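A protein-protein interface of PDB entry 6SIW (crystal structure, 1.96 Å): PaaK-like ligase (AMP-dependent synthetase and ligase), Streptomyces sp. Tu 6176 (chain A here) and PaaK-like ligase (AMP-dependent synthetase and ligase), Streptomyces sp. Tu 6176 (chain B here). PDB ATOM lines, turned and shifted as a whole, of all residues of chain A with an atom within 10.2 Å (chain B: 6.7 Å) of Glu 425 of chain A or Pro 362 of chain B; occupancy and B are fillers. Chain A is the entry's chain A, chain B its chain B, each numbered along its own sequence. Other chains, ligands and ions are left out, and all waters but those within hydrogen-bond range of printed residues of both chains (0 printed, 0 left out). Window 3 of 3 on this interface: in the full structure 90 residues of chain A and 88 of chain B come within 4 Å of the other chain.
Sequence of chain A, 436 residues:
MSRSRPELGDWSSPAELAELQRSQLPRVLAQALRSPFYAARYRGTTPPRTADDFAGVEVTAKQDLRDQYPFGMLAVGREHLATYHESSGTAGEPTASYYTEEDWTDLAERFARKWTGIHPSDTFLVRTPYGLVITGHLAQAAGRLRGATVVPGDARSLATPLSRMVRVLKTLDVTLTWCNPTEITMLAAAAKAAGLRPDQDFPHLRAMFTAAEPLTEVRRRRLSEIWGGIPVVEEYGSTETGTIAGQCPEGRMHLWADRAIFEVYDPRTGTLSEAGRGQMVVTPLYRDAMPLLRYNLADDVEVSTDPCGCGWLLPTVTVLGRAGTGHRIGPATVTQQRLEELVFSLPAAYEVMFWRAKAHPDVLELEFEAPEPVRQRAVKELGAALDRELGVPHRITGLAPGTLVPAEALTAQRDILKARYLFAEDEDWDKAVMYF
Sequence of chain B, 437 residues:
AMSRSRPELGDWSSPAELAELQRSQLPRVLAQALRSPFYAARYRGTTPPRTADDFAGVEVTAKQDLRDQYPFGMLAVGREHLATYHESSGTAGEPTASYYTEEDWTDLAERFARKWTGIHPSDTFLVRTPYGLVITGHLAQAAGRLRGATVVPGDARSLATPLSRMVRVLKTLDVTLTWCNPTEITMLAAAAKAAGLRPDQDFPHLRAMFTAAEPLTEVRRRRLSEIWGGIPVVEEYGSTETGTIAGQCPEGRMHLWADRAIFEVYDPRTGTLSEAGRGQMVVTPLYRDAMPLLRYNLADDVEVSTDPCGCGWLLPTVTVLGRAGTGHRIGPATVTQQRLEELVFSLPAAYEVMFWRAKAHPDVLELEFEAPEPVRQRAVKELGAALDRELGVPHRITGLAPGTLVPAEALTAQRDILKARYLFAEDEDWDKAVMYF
The backbone carbonyl oxygen (O) of Phe 423 of chain A lies within hydrogen-bond range of the backbone NH (N) of Ala 360 of chain B, 2.7 Å away. O of Ala 360 of chain B lies within hydrogen-bond range of N of Glu 425 of chain A (3.2 Å). A ring nitrogen (ND1) of His 361 of chain B lies within hydrogen-bond range of the side-chain carboxylate of Glu 425 of chain A (3.1 Å).
Printed residues of chain B within 4 Å of Ala 424 of chain A: His 328 (3.6 Å), Lys 359 (3.7 Å) and Ala 360 (3.97 Å). Glu 425 of chain A touches just these residues of chain B: Lys 359 (3.8 Å), Ala 360 (3.2 Å), His 361 (3.1 Å) and Pro 362 (3.0 Å). Printed residues of chain B within 4 Å of Glu 427 of chain A: Lys 359 (3.9 Å). Printed residues of chain B within 4 Å of Trp 429 of chain A: Lys 359. Of the printed residues of chain A, Lys 359 of chain B touches Phe 423 (3.3 Å), Ala 424 (3.7 Å), Glu 425 (3.8 Å), Glu 427 (3.9 Å) and Trp 429 (3.8 Å). Ala 360 of chain B touches just these residues of chain A: Phe 423, Ala 424 and Glu 425. His 361 of chain B touches just one residue of chain A: Glu 425. Printed residues of chain A within 4 Å of Pro 362 of chain B: Glu 425. No residue of chain A comes within 4 Å of Asp 363 of chain B. The nearest residue of chain A that does not touch Pro 362 of chain B is Ala 424 of chain A (7.5 Å). The nearest printed residue of chain B that does not touch Trp 429 of chain A is His 361 of chain B (6.6 Å).
Of the 11 printed residues of chain B, 5 touch a printed residue of chain A. Hydrophobic or aromatic side chains of chain A that line the printed part of chain B: Leu 422, Ala 424 and Trp 429. Among the printed residues, 13 pairs touch across the chains. Among the printed residues, no Asp or Glu carboxylate lies within 4 Å of a Lys or Arg side-chain nitrogen of the other chain.
The guanidinium group of Arg 420 of chain A is in hydrogen-bond range of the backbone carbonyl oxygen of Leu 422 of chain A, at 3.0 Å. The guanidinium group of Arg 420 of chain A is in salt-bridge range of the side-chain carboxylate of Glu 427 of chain A. OE1 of Glu 427 of chain A lies within hydrogen-bond range of N of Ala 424 of chain A.
Among the printed residues, merely in contact across the chains: Glu 425 of chain A with Pro 362 of chain B (3.0 Å), Phe 423 of chain A with Lys 359 of chain B (3.3 Å), Leu 422 of chain A with His 328 of chain B (3.6 Å), Ala 424 of chain A with His 328 of chain B (3.6 Å), Ala 424 of chain A with Lys 359 of chain B (3.7 Å), Trp 429 of chain A with Lys 359 of chain B (3.8 Å), Glu 425 of chain A with Lys 359 of chain B (3.8 Å), Glu 427 of chain A with Lys 359 of chain B (3.9 Å), Phe 423 of chain A with His 328 of chain B (3.9 Å) and Ala 424 of chain A with Ala 360 of chain B (3.97 Å).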
ATOM      1  N   ARG A 420      20.260 -18.467  -6.005  1.00  0.00           N
ATOM      2  CA  ARG A 420      19.438 -19.100  -7.053  1.00  0.00           C
ATOM      3  C   ARG A 420      20.381 -19.421  -8.196  1.00  0.00           C
ATOM      4  O   ARG A 420      21.306 -18.657  -8.430  1.00  0.00           O
ATOM      5  CB  ARG A 420      18.281 -18.183  -7.439  1.00  0.00           C
ATOM      6  CG  ARG A 420      17.166 -18.180  -6.403  1.00  0.00           C
ATOM      7  CD  ARG A 420      15.930 -17.459  -6.905  1.00  0.00           C
ATOM      8  NE  ARG A 420      15.472 -18.098  -8.127  1.00  0.00           N
ATOM      9  CZ  ARG A 420      14.921 -17.474  -9.164  1.00  0.00           C
ATOM     10  NH1 ARG A 420      14.726 -16.166  -9.150  1.00  0.00           N
ATOM     11  NH2 ARG A 420      14.572 -18.180 -10.224  1.00  0.00           N
ATOM     12  N   LEU A 422      19.054 -21.458 -11.219  1.00  0.00           N
ATOM     13  CA  LEU A 422      18.176 -21.521 -12.412  1.00  0.00           C
ATOM     14  C   LEU A 422      17.249 -20.302 -12.452  1.00  0.00           C
ATOM     15  O   LEU A 422      16.528 -20.062 -11.474  1.00  0.00           O
ATOM     16  CB  LEU A 422      17.381 -22.821 -12.343  1.00  0.00           C
ATOM     17  CG  LEU A 422      16.483 -23.090 -13.542  1.00  0.00           C
ATOM     18  CD1 LEU A 422      17.257 -22.961 -14.852  1.00  0.00           C
ATOM     19  CD2 LEU A 422      15.860 -24.469 -13.428  1.00  0.00           C
ATOM     20  N   PHE A 423      17.261 -19.570 -13.565  1.00  0.00           N
ATOM     21  CA  PHE A 423      16.458 -18.342 -13.779  1.00  0.00           C
ATOM     22  C   PHE A 423      15.554 -18.517 -14.999  1.00  0.00           C
ATOM     23  O   PHE A 423      15.878 -19.271 -15.924  1.00  0.00           O
ATOM     24  CB  PHE A 423      17.376 -17.133 -13.940  1.00  0.00           C
ATOM     25  CG  PHE A 423      18.150 -16.820 -12.689  1.00  0.00           C
ATOM     26  CD1 PHE A 423      19.343 -17.469 -12.415  1.00  0.00           C
ATOM     27  CD2 PHE A 423      17.660 -15.905 -11.769  1.00  0.00           C
ATOM     28  CE1 PHE A 423      20.040 -17.197 -11.250  1.00  0.00           C
ATOM     29  CE2 PHE A 423      18.359 -15.628 -10.607  1.00  0.00           C
ATOM     30  CZ  PHE A 423      19.545 -16.284 -10.347  1.00  0.00           C
ATOM     31  N   ALA A 424      14.414 -17.836 -14.970  1.00  0.00           N
ATOM     32  CA  ALA A 424      13.511 -17.665 -16.124  1.00  0.00           C
ATOM     33  C   ALA A 424      14.131 -16.619 -17.050  1.00  0.00           C
ATOM     34  O   ALA A 424      14.901 -15.758 -16.557  1.00  0.00           O
ATOM     35  CB  ALA A 424      12.138 -17.257 -15.651  1.00  0.00           C
ATOM     36  N   GLU A 425      13.790 -16.698 -18.336  1.00  0.00           N
ATOM     37  CA  GLU A 425      14.312 -15.841 -19.435  1.00  0.00           C
ATOM     38  C   GLU A 425      14.298 -14.362 -19.023  1.00  0.00           C
ATOM     39  O   GLU A 425      15.281 -13.661 -19.325  1.00  0.00           O
ATOM     40  CB  GLU A 425      13.478 -16.108 -20.688  1.00  0.00           C
ATOM     41  CG  GLU A 425      13.644 -15.076 -21.785  1.00  0.00           C
ATOM     42  CD  GLU A 425      13.115 -15.536 -23.138  1.00  0.00           C
ATOM     43  OE1 GLU A 425      13.643 -16.537 -23.674  1.00  0.00           O
ATOM     44  OE2 GLU A 425      12.174 -14.898 -23.657  1.00  0.00           O
ATOM     45  N   ASP A 426      13.243 -13.912 -18.339  1.00  0.00           N
ATOM     46  CA  ASP A 426      12.969 -12.476 -18.053  1.00  0.00           C
ATOM     47  C   ASP A 426      13.631 -12.010 -16.744  1.00  0.00           C
ATOM     48  O   ASP A 426      13.408 -10.832 -16.381  1.00  0.00           O
ATOM     49  CB  ASP A 426      11.462 -12.219 -17.979  1.00  0.00           C
ATOM     50  CG  ASP A 426      10.771 -12.984 -16.860  1.00  0.00           C
ATOM     51  OD1 ASP A 426      10.829 -14.232 -16.875  1.00  0.00           O
ATOM     52  OD2 ASP A 426      10.191 -12.329 -15.978  1.00  0.00           O
ATOM     53  N   GLU A 427      14.400 -12.858 -16.051  1.00  0.00           N
ATOM     54  CA  GLU A 427      14.988 -12.505 -14.727  1.00  0.00           C
ATOM     55  C   GLU A 427      16.427 -12.012 -14.891  1.00  0.00           C
ATOM     56  O   GLU A 427      17.070 -12.361 -15.907  1.00  0.00           O
ATOM     57  CB  GLU A 427      14.967 -13.696 -13.779  1.00  0.00           C
ATOM     58  CG  GLU A 427      13.572 -14.161 -13.445  1.00  0.00           C
ATOM     59  CD  GLU A 427      13.540 -15.141 -12.290  1.00  0.00           C
ATOM     60  OE1 GLU A 427      13.431 -16.351 -12.556  1.00  0.00           O
ATOM     61  OE2 GLU A 427      13.632 -14.684 -11.134  1.00  0.00           O
ATOM     62  N   ASP A 428      16.896 -11.243 -13.904  1.00  0.00           N
ATOM     63  CA  ASP A 428      18.302 -10.780 -13.782  1.00  0.00           C
ATOM     64  C   ASP A 428      19.121 -11.869 -13.078  1.00  0.00           C
ATOM     65  O   ASP A 428      19.058 -11.953 -11.828  1.00  0.00           O
ATOM     66  CB  ASP A 428      18.372  -9.450 -13.034  1.00  0.00           C
ATOM     67  CG  ASP A 428      19.674  -8.706 -13.266  1.00  0.00           C
ATOM     68  OD1 ASP A 428      20.692  -9.378 -13.512  1.00  0.00           O
ATOM     69  OD2 ASP A 428      19.651  -7.465 -13.219  1.00  0.00           O
ATOM     70  N   TRP A 429      19.864 -12.678 -13.843  1.00  0.00           N
ATOM     71  CA  TRP A 429      20.637 -13.828 -13.298  1.00  0.00           C
ATOM     72  C   TRP A 429      22.007 -13.372 -12.783  1.00  0.00           C
ATOM     73  O   TRP A 429      22.804 -14.259 -12.408  1.00  0.00           O
ATOM     74  CB  TRP A 429      20.750 -14.978 -14.304  1.00  0.00           C
ATOM     75  CG  TRP A 429      21.681 -14.758 -15.451  1.00  0.00           C
ATOM     76  CD1 TRP A 429      22.124 -13.569 -15.951  1.00  0.00           C
ATOM     77  CD2 TRP A 429      22.246 -15.780 -16.282  1.00  0.00           C
ATOM     78  NE1 TRP A 429      22.925 -13.783 -17.037  1.00  0.00           N
ATOM     79  CE2 TRP A 429      23.020 -15.129 -17.267  1.00  0.00           C
ATOM     80  CE3 TRP A 429      22.183 -17.179 -16.288  1.00  0.00           C
ATOM     81  CZ2 TRP A 429      23.736 -15.831 -18.232  1.00  0.00           C
ATOM     82  CZ3 TRP A 429      22.873 -17.871 -17.254  1.00  0.00           C
ATOM     83  CH2 TRP A 429      23.641 -17.205 -18.211  1.00  0.00           C
ATOM     84  N   ASP A 430      22.247 -12.058 -12.692  1.00  0.00           N
ATOM     85  CA  ASP A 430      23.442 -11.486 -12.013  1.00  0.00           C
ATOM     86  C   ASP A 430      23.210 -11.483 -10.488  1.00  0.00           C
ATOM     87  O   ASP A 430      23.936 -10.764  -9.769  1.00  0.00           O
ATOM     88  CB  ASP A 430      23.781 -10.095 -12.564  1.00  0.00           C
ATOM     89  CG  ASP A 430      24.218 -10.069 -14.025  1.00  0.00           C
ATOM     90  OD1 ASP A 430      24.903 -11.015 -14.483  1.00  0.00           O
ATOM     91  OD2 ASP A 430      23.876  -9.088 -14.701  1.00  0.00           O
ATOM     92  N   HIS B 328      10.318 -24.878 -14.662  1.00  0.00           N
ATOM     93  CA  HIS B 328      10.530 -24.369 -16.045  1.00  0.00           C
ATOM     94  C   HIS B 328      10.418 -25.527 -17.031  1.00  0.00           C
ATOM     95  O   HIS B 328      10.977 -26.593 -16.769  1.00  0.00           O
ATOM     96  CB  HIS B 328      11.886 -23.672 -16.226  1.00  0.00           C
ATOM     97  CG  HIS B 328      12.205 -22.689 -15.156  1.00  0.00           C
ATOM     98  ND1 HIS B 328      12.017 -21.330 -15.321  1.00  0.00           N
ATOM     99  CD2 HIS B 328      12.689 -22.871 -13.904  1.00  0.00           C
ATOM    100  CE1 HIS B 328      12.376 -20.715 -14.209  1.00  0.00           C
ATOM    101  NE2 HIS B 328      12.793 -21.636 -13.325  1.00  0.00           N
ATOM    102  N   ARG B 329       9.673 -25.319 -18.106  1.00  0.00           N
ATOM    103  CA  ARG B 329       9.523 -26.301 -19.200  1.00  0.00           C
ATOM    104  C   ARG B 329      10.328 -25.761 -20.378  1.00  0.00           C
ATOM    105  O   ARG B 329      10.217 -24.561 -20.669  1.00  0.00           O
ATOM    106  CB  ARG B 329       8.034 -26.543 -19.454  1.00  0.00           C
ATOM    107  CG  ARG B 329       7.375 -27.271 -18.293  1.00  0.00           C
ATOM    108  CD  ARG B 329       5.873 -27.396 -18.405  1.00  0.00           C
ATOM    109  NE  ARG B 329       5.332 -28.420 -17.516  1.00  0.00           N
ATOM    110  CZ  ARG B 329       5.130 -28.287 -16.199  1.00  0.00           C
ATOM    111  NH1 ARG B 329       4.623 -29.302 -15.518  1.00  0.00           N
ATOM    112  NH2 ARG B 329       5.439 -27.163 -15.567  1.00  0.00           N
ATOM    113  N   ILE B 330      11.151 -26.617 -20.981  1.00  0.00           N
ATOM    114  CA  ILE B 330      11.892 -26.341 -22.244  1.00  0.00           C
ATOM    115  C   ILE B 330      11.518 -27.463 -23.216  1.00  0.00           C
ATOM    116  O   ILE B 330      12.030 -28.589 -23.057  1.00  0.00           O
ATOM    117  CB  ILE B 330      13.401 -26.234 -21.971  1.00  0.00           C
ATOM    118  CG1 ILE B 330      13.692 -25.044 -21.054  1.00  0.00           C
ATOM    119  CG2 ILE B 330      14.200 -26.184 -23.269  1.00  0.00           C
ATOM    120  CD1 ILE B 330      15.166 -24.772 -20.819  1.00  0.00           C
ATOM    121  N   GLY B 331      10.612 -27.157 -24.154  1.00  0.00           N
ATOM    122  CA  GLY B 331       9.761 -28.154 -24.822  1.00  0.00           C
ATOM    123  C   GLY B 331       9.035 -28.991 -23.770  1.00  0.00           C
ATOM    124  O   GLY B 331       8.481 -28.455 -22.805  1.00  0.00           O
ATOM    125  N   LYS B 359      19.826 -20.173 -17.352  1.00  0.00           N
ATOM    126  CA  LYS B 359      18.592 -19.454 -17.743  1.00  0.00           C
ATOM    127  C   LYS B 359      17.756 -20.385 -18.609  1.00  0.00           C
ATOM    128  O   LYS B 359      18.287 -20.907 -19.610  1.00  0.00           O
ATOM    129  CB  LYS B 359      18.917 -18.148 -18.468  1.00  0.00           C
ATOM    130  CG  LYS B 359      17.800 -17.115 -18.433  1.00  0.00           C
ATOM    131  CD  LYS B 359      18.271 -15.715 -18.049  1.00  0.00           C
ATOM    132  CE  LYS B 359      19.118 -15.067 -19.121  1.00  0.00           C
ATOM    133  NZ  LYS B 359      19.393 -13.647 -18.814  1.00  0.00           N
ATOM    134  N   ALA B 360      16.522 -20.642 -18.187  1.00  0.00           N
ATOM    135  CA  ALA B 360      15.526 -21.421 -18.964  1.00  0.00           C
ATOM    136  C   ALA B 360      14.885 -20.483 -19.990  1.00  0.00           C
ATOM    137  O   ALA B 360      14.050 -19.655 -19.600  1.00  0.00           O
ATOM    138  CB  ALA B 360      14.498 -22.057 -18.048  1.00  0.00           C
ATOM    139  N   HIS B 361      15.325 -20.556 -21.242  1.00  0.00           N
ATOM    140  CA  HIS B 361      14.623 -19.947 -22.407  1.00  0.00           C
ATOM    141  C   HIS B 361      13.602 -20.956 -22.925  1.00  0.00           C
ATOM    142  O   HIS B 361      13.766 -22.158 -22.718  1.00  0.00           O
ATOM    143  CB  HIS B 361      15.601 -19.526 -23.521  1.00  0.00           C
ATOM    144  CG  HIS B 361      16.705 -18.638 -23.059  1.00  0.00           C
ATOM    145  ND1 HIS B 361      16.540 -17.278 -22.895  1.00  0.00           N
ATOM    146  CD2 HIS B 361      17.984 -18.907 -22.713  1.00  0.00           C
ATOM    147  CE1 HIS B 361      17.666 -16.750 -22.463  1.00  0.00           C
ATOM    148  NE2 HIS B 361      18.569 -17.728 -22.350  1.00  0.00           N
ATOM    149  N   PRO B 362      12.526 -20.519 -23.620  1.00  0.00           N
ATOM    150  CA  PRO B 362      11.560 -21.449 -24.214  1.00  0.00           C
ATOM    151  C   PRO B 362      12.209 -22.524 -25.105  1.00  0.00           C
ATOM    152  O   PRO B 362      11.720 -23.627 -25.143  1.00  0.00           O
ATOM    153  CB  PRO B 362      10.658 -20.551 -25.079  1.00  0.00           C
ATOM    154  CG  PRO B 362      10.781 -19.170 -24.457  1.00  0.00           C
ATOM    155  CD  PRO B 362      12.172 -19.113 -23.853  1.00  0.00           C
ATOM    156  N   ASP B 363      13.314 -22.180 -25.767  1.00  0.00           N
ATOM    157  CA  ASP B 363      13.939 -22.991 -26.845  1.00  0.00           C
ATOM    158  C   ASP B 363      15.237 -23.666 -26.371  1.00  0.00           C
ATOM    159  O   ASP B 363      15.654 -24.635 -27.033  1.00  0.00           O
ATOM    160  CB  ASP B 363      14.204 -22.118 -28.080  1.00  0.00           C
ATOM    161  CG  ASP B 363      14.970 -20.829 -27.805  1.00  0.00           C
ATOM    162  OD1 ASP B 363      14.767 -20.234 -26.723  1.00  0.00           O
ATOM    163  OD2 ASP B 363      15.755 -20.420 -28.683  1.00  0.00           O
ATOM    164  N   VAL B 364      15.893 -23.174 -25.312  1.00  0.00           N
ATOM    165  CA  VAL B 364      17.304 -23.573 -25.014  1.00  0.00           C
ATOM    166  C   VAL B 364      17.655 -23.274 -23.549  1.00  0.00           C
ATOM    167  O   VAL B 364      17.166 -22.273 -22.992  1.00  0.00           O
ATOM    168  CB  VAL B 364      18.287 -22.891 -25.996  1.00  0.00           C
ATOM    169  CG1 VAL B 364      18.421 -21.395 -25.736  1.00  0.00           C
ATOM    170  CG2 VAL B 364      19.650 -23.574 -26.007  1.00  0.00           C
ATOM    171  N   PRO B 394      17.952 -28.876 -25.580  1.00  0.00           N
ATOM    172  CA  PRO B 394      18.995 -28.120 -26.263  1.00  0.00           C
ATOM    173  C   PRO B 394      19.606 -27.147 -25.244  1.00  0.00           C
ATOM    174  O   PRO B 394      18.888 -26.621 -24.401  1.00  0.00           O
ATOM    175  CB  PRO B 394      18.276 -27.430 -27.433  1.00  0.00           C
ATOM    176  CG  PRO B 394      16.824 -27.382 -27.013  1.00  0.00           C
ATOM    177  CD  PRO B 394      16.611 -28.565 -26.089  1.00  0.00           C
